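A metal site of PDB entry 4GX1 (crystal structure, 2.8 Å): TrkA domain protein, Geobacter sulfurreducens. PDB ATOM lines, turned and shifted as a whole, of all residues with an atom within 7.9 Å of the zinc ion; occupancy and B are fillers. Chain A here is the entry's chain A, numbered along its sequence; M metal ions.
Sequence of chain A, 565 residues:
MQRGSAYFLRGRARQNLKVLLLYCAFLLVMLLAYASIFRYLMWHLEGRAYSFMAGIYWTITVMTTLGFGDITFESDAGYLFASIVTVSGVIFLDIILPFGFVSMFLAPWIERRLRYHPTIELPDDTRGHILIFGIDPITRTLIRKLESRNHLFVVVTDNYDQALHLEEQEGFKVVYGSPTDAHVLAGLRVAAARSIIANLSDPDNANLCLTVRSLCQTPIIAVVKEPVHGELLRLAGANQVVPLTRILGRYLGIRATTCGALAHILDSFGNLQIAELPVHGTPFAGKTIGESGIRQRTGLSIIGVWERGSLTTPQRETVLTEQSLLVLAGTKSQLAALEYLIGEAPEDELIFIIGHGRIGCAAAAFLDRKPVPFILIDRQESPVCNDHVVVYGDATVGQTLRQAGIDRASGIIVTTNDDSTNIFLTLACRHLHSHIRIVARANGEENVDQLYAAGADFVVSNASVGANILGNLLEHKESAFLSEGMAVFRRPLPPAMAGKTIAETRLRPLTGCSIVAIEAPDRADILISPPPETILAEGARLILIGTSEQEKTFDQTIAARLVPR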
ATOM      1  N   HIS A 356      17.253  -7.890  15.994  1.00  0.00           N
ATOM      2  CA  HIS A 356      15.958  -7.218  15.978  1.00  0.00           C
ATOM      3  C   HIS A 356      15.420  -7.019  17.385  1.00  0.00           C
ATOM      4  O   HIS A 356      14.280  -7.351  17.685  1.00  0.00           O
ATOM      5  CB  HIS A 356      14.960  -8.001  15.126  1.00  0.00           C
ATOM      6  CG  HIS A 356      13.625  -7.338  15.002  1.00  0.00           C
ATOM      7  ND1 HIS A 356      12.456  -7.951  15.412  1.00  0.00           N
ATOM      8  CD2 HIS A 356      13.274  -6.125  14.532  1.00  0.00           C
ATOM      9  CE1 HIS A 356      11.441  -7.129  15.181  1.00  0.00           C
ATOM     10  NE2 HIS A 356      11.912  -6.018  14.652  1.00  0.00           N
ATOM     11  N   GLY A 357      16.267  -6.485  18.259  1.00  0.00           N
ATOM     12  CA  GLY A 357      15.813  -6.056  19.569  1.00  0.00           C
ATOM     13  C   GLY A 357      15.228  -4.664  19.432  1.00  0.00           C
ATOM     14  O   GLY A 357      14.857  -4.248  18.333  1.00  0.00           O
ATOM     15  N   ARG A 358      15.160  -3.927  20.530  1.00  0.00           N
ATOM     16  CA  ARG A 358      14.523  -2.624  20.511  1.00  0.00           C
ATOM     17  C   ARG A 358      15.266  -1.597  19.655  1.00  0.00           C
ATOM     18  O   ARG A 358      14.642  -0.770  18.983  1.00  0.00           O
ATOM     19  CB  ARG A 358      14.330  -2.110  21.936  1.00  0.00           C
ATOM     20  CG  ARG A 358      13.205  -2.812  22.675  1.00  0.00           C
ATOM     21  CD  ARG A 358      12.750  -1.984  23.874  1.00  0.00           C
ATOM     22  NE  ARG A 358      11.450  -2.411  24.373  1.00  0.00           N
ATOM     23  CZ  ARG A 358      11.233  -2.946  25.583  1.00  0.00           C
ATOM     24  NH1 ARG A 358      12.250  -3.112  26.425  1.00  0.00           N
ATOM     25  NH2 ARG A 358      10.006  -3.304  25.930  1.00  0.00           N
ATOM     26  N   GLY A 360      17.686  -2.245  17.074  1.00  0.00           N
ATOM     27  CA  GLY A 360      17.683  -2.704  15.698  1.00  0.00           C
ATOM     28  C   GLY A 360      16.334  -2.424  15.077  1.00  0.00           C
ATOM     29  O   GLY A 360      16.221  -2.066  13.908  1.00  0.00           O
ATOM     30  N   CYS A 361      15.296  -2.605  15.882  1.00  0.00           N
ATOM     31  CA  CYS A 361      13.954  -2.226  15.493  1.00  0.00           C
ATOM     32  C   CYS A 361      13.865  -0.732  15.165  1.00  0.00           C
ATOM     33  O   CYS A 361      13.301  -0.344  14.151  1.00  0.00           O
ATOM     34  CB  CYS A 361      12.984  -2.562  16.618  1.00  0.00           C
ATOM     35  SG  CYS A 361      11.264  -2.311  16.187  1.00  0.00           S
ATOM     36  N   ALA A 362      14.422   0.097  16.044  1.00  0.00           N
ATOM     37  CA  ALA A 362      14.432   1.547  15.861  1.00  0.00           C
ATOM     38  C   ALA A 362      15.159   1.947  14.563  1.00  0.00           C
ATOM     39  O   ALA A 362      14.729   2.857  13.850  1.00  0.00           O
ATOM     40  CB  ALA A 362      15.065   2.247  17.071  1.00  0.00           C
ATOM     41  N   ALA A 364      15.420  -0.017  11.855  1.00  0.00           N
ATOM     42  CA  ALA A 364      14.541  -0.404  10.754  1.00  0.00           C
ATOM     43  C   ALA A 364      13.335   0.521  10.669  1.00  0.00           C
ATOM     44  O   ALA A 364      12.818   0.784   9.583  1.00  0.00           O
ATOM     45  CB  ALA A 364      14.108  -1.855  10.901  1.00  0.00           C
ATOM     46  N   ALA A 365      12.880   0.999  11.824  1.00  0.00           N
ATOM     47  CA  ALA A 365      11.782   1.955  11.856  1.00  0.00           C
ATOM     48  C   ALA A 365      12.229   3.247  11.173  1.00  0.00           C
ATOM     49  O   ALA A 365      11.432   3.930  10.544  1.00  0.00           O
ATOM     50  CB  ALA A 365      11.359   2.223  13.272  1.00  0.00           C
ATOM     51  N   ASP A 368      12.561   2.786   7.313  1.00  0.00           N
ATOM     52  CA  ASP A 368      11.226   2.737   6.721  1.00  0.00           C
ATOM     53  C   ASP A 368      10.839   4.114   6.175  1.00  0.00           C
ATOM     54  O   ASP A 368      10.217   4.211   5.117  1.00  0.00           O
ATOM     55  CB  ASP A 368      10.185   2.292   7.752  1.00  0.00           C
ATOM     56  CG  ASP A 368       9.942   0.793   7.724  1.00  0.00           C
ATOM     57  OD1 ASP A 368       9.854   0.211   6.615  1.00  0.00           O
ATOM     58  OD2 ASP A 368       9.847   0.185   8.816  1.00  0.00           O
ATOM     59  N   PHE A 374      15.456  -3.097   3.779  1.00  0.00           N
ATOM     60  CA  PHE A 374      16.376  -3.731   4.710  1.00  0.00           C
ATOM     61  C   PHE A 374      15.974  -5.163   4.982  1.00  0.00           C
ATOM     62  O   PHE A 374      14.895  -5.598   4.580  1.00  0.00           O
ATOM     63  CB  PHE A 374      16.396  -2.960   6.039  1.00  0.00           C
ATOM     64  CG  PHE A 374      15.030  -2.725   6.610  1.00  0.00           C
ATOM     65  CD1 PHE A 374      14.377  -3.723   7.312  1.00  0.00           C
ATOM     66  CD2 PHE A 374      14.395  -1.503   6.448  1.00  0.00           C
ATOM     67  CE1 PHE A 374      13.113  -3.510   7.840  1.00  0.00           C
ATOM     68  CE2 PHE A 374      13.125  -1.278   6.975  1.00  0.00           C
ATOM     69  CZ  PHE A 374      12.494  -2.280   7.677  1.00  0.00           C
ATOM     70  N   LEU A 376      15.913  -7.801   8.416  1.00  0.00           N
ATOM     71  CA  LEU A 376      16.147  -8.055   9.834  1.00  0.00           C
ATOM     72  C   LEU A 376      16.427  -9.529  10.105  1.00  0.00           C
ATOM     73  O   LEU A 376      15.697 -10.409   9.650  1.00  0.00           O
ATOM     74  CB  LEU A 376      14.932  -7.632  10.656  1.00  0.00           C
ATOM     75  CG  LEU A 376      14.740  -6.125  10.731  1.00  0.00           C
ATOM     76  CD1 LEU A 376      13.306  -5.808  11.134  1.00  0.00           C
ATOM     77  CD2 LEU A 376      15.744  -5.529  11.714  1.00  0.00           C
ATOM     78  N   SER A 382      10.242 -11.225  18.155  1.00  0.00           N
ATOM     79  CA  SER A 382      10.115 -10.098  19.070  1.00  0.00           C
ATOM     80  C   SER A 382       8.839 -10.187  19.906  1.00  0.00           C
ATOM     81  O   SER A 382       7.765 -10.500  19.385  1.00  0.00           O
ATOM     82  CB  SER A 382      10.117  -8.778  18.308  1.00  0.00           C
ATOM     83  OG  SER A 382       9.676  -7.716  19.129  1.00  0.00           O
ATOM     84  N   VAL A 384       7.580  -7.601  21.602  1.00  0.00           N
ATOM     85  CA  VAL A 384       6.943  -6.291  21.644  1.00  0.00           C
ATOM     86  C   VAL A 384       6.571  -5.759  20.266  1.00  0.00           C
ATOM     87  O   VAL A 384       5.796  -4.821  20.155  1.00  0.00           O
ATOM     88  CB  VAL A 384       7.819  -5.240  22.335  1.00  0.00           C
ATOM     89  CG1 VAL A 384       8.287  -5.744  23.698  1.00  0.00           C
ATOM     90  CG2 VAL A 384       9.011  -4.893  21.454  1.00  0.00           C
ATOM     91  N   CYS A 385       7.129  -6.364  19.228  1.00  0.00           N
ATOM     92  CA  CYS A 385       6.909  -5.871  17.865  1.00  0.00           C
ATOM     93  C   CYS A 385       6.258  -6.865  16.903  1.00  0.00           C
ATOM     94  O   CYS A 385       6.459  -8.084  16.986  1.00  0.00           O
ATOM     95  CB  CYS A 385       8.204  -5.350  17.252  1.00  0.00           C
ATOM     96  SG  CYS A 385       8.005  -4.940  15.516  1.00  0.00           S
ATOM     97  N   ASN A 386       5.493  -6.323  15.950  1.00  0.00           N
ATOM     98  CA  ASN A 386       4.895  -7.119  14.886  1.00  0.00           C
ATOM     99  C   ASN A 386       4.542  -6.278  13.665  1.00  0.00           C
ATOM    100  O   ASN A 386       3.565  -6.549  12.970  1.00  0.00           O
ATOM    101  CB  ASN A 386       3.668  -7.878  15.411  1.00  0.00           C
ATOM    102  CG  ASN A 386       2.710  -7.000  16.170  1.00  0.00           C
ATOM    103  OD1 ASN A 386       3.105  -5.974  16.747  1.00  0.00           O
ATOM    104  ND2 ASN A 386       1.444  -7.376  16.180  1.00  0.00           N
ATOM    105  N   ASP A 387       5.349  -5.251  13.403  1.00  0.00           N
ATOM    106  CA  ASP A 387       5.176  -4.406  12.228  1.00  0.00           C
ATOM    107  C   ASP A 387       6.245  -4.736  11.202  1.00  0.00           C
ATOM    108  O   ASP A 387       6.140  -4.381  10.029  1.00  0.00           O
ATOM    109  CB  ASP A 387       5.270  -2.923  12.601  1.00  0.00           C
ATOM    110  CG  ASP A 387       4.350  -2.542  13.756  1.00  0.00           C
ATOM    111  OD1 ASP A 387       3.714  -1.471  13.681  1.00  0.00           O
ATOM    112  OD2 ASP A 387       4.284  -3.292  14.757  1.00  0.00           O
ATOM    113  N   HIS A 388       7.304  -5.403  11.659  1.00  0.00           N
ATOM    114  CA  HIS A 388       8.451  -5.724  10.804  1.00  0.00           C
ATOM    115  C   HIS A 388       8.515  -7.222  10.499  1.00  0.00           C
ATOM    116  O   HIS A 388       8.136  -8.049  11.331  1.00  0.00           O
ATOM    117  CB  HIS A 388       9.761  -5.282  11.469  1.00  0.00           C
ATOM    118  CG  HIS A 388      10.022  -3.811  11.378  1.00  0.00           C
ATOM    119  ND1 HIS A 388      10.617  -3.085  12.389  1.00  0.00           N
ATOM    120  CD2 HIS A 388       9.783  -2.923  10.379  1.00  0.00           C
ATOM    121  CE1 HIS A 388      10.721  -1.820  12.030  1.00  0.00           C
ATOM    122  NE2 HIS A 388      10.221  -1.694  10.809  1.00  0.00           N
ATOM    123  N   VAL A 389       8.979  -7.562   9.306  1.00  0.00           N
ATOM    124  CA  VAL A 389       9.209  -8.959   8.937  1.00  0.00           C
ATOM    125  C   VAL A 389      10.650  -9.337   9.279  1.00  0.00           C
ATOM    126  O   VAL A 389      11.592  -8.643   8.907  1.00  0.00           O
ATOM    127  CB  VAL A 389       8.928  -9.207   7.418  1.00  0.00           C
ATOM    128  CG1 VAL A 389       9.663 -10.436   6.906  1.00  0.00           C
ATOM    129  CG2 VAL A 389       7.436  -9.338   7.171  1.00  0.00           C
ATOM    130  N   VAL A 390      10.797 -10.448  10.006  1.00  0.00           N
ATOM    131  CA  VAL A 390      12.112 -10.880  10.483  1.00  0.00           C
ATOM    132  C   VAL A 390      12.477 -12.273   9.975  1.00  0.00           C
ATOM    133  O   VAL A 390      11.643 -13.181   9.977  1.00  0.00           O
ATOM    134  CB  VAL A 390      12.170 -10.891  12.018  1.00  0.00           C
ATOM    135  CG1 VAL A 390      13.510 -11.390  12.509  1.00  0.00           C
ATOM    136  CG2 VAL A 390      11.873  -9.515  12.570  1.00  0.00           C
HETATM  137 ZN    ZN M   1      10.368  -4.152  14.622  1.00  0.00          ZN
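The backbone NH (N) of Cys 385 lies within hydrogen-bond range of the side-chain hydroxyl (OG) of Ser 382, 2.9 Å away. The side-chain sulfur (SG) of Cys 385 lies close to the backbone NH (N) of Asp 387, at 3.4 Å. NE2 of His 388 sits at hydrogen-bond distance from OD2 of Asp 368, at 2.8 Å.
Within 4 Å of the zinc ion: His 356, Cys 361, Cys 385 and His 388. The nearest printed residue that does not touch the zinc ion is Leu 376 (4.9 Å).
The zinc ion is bound by a ring nitrogen (NE2) of His 356 (2.4 Å), a ring nitrogen (ND1) of His 388 (2.5 Å), the side-chain sulfur (SG) of Cys 361 (2.6 Å) and the side-chain sulfur (SG) of Cys 385 (2.6 Å).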
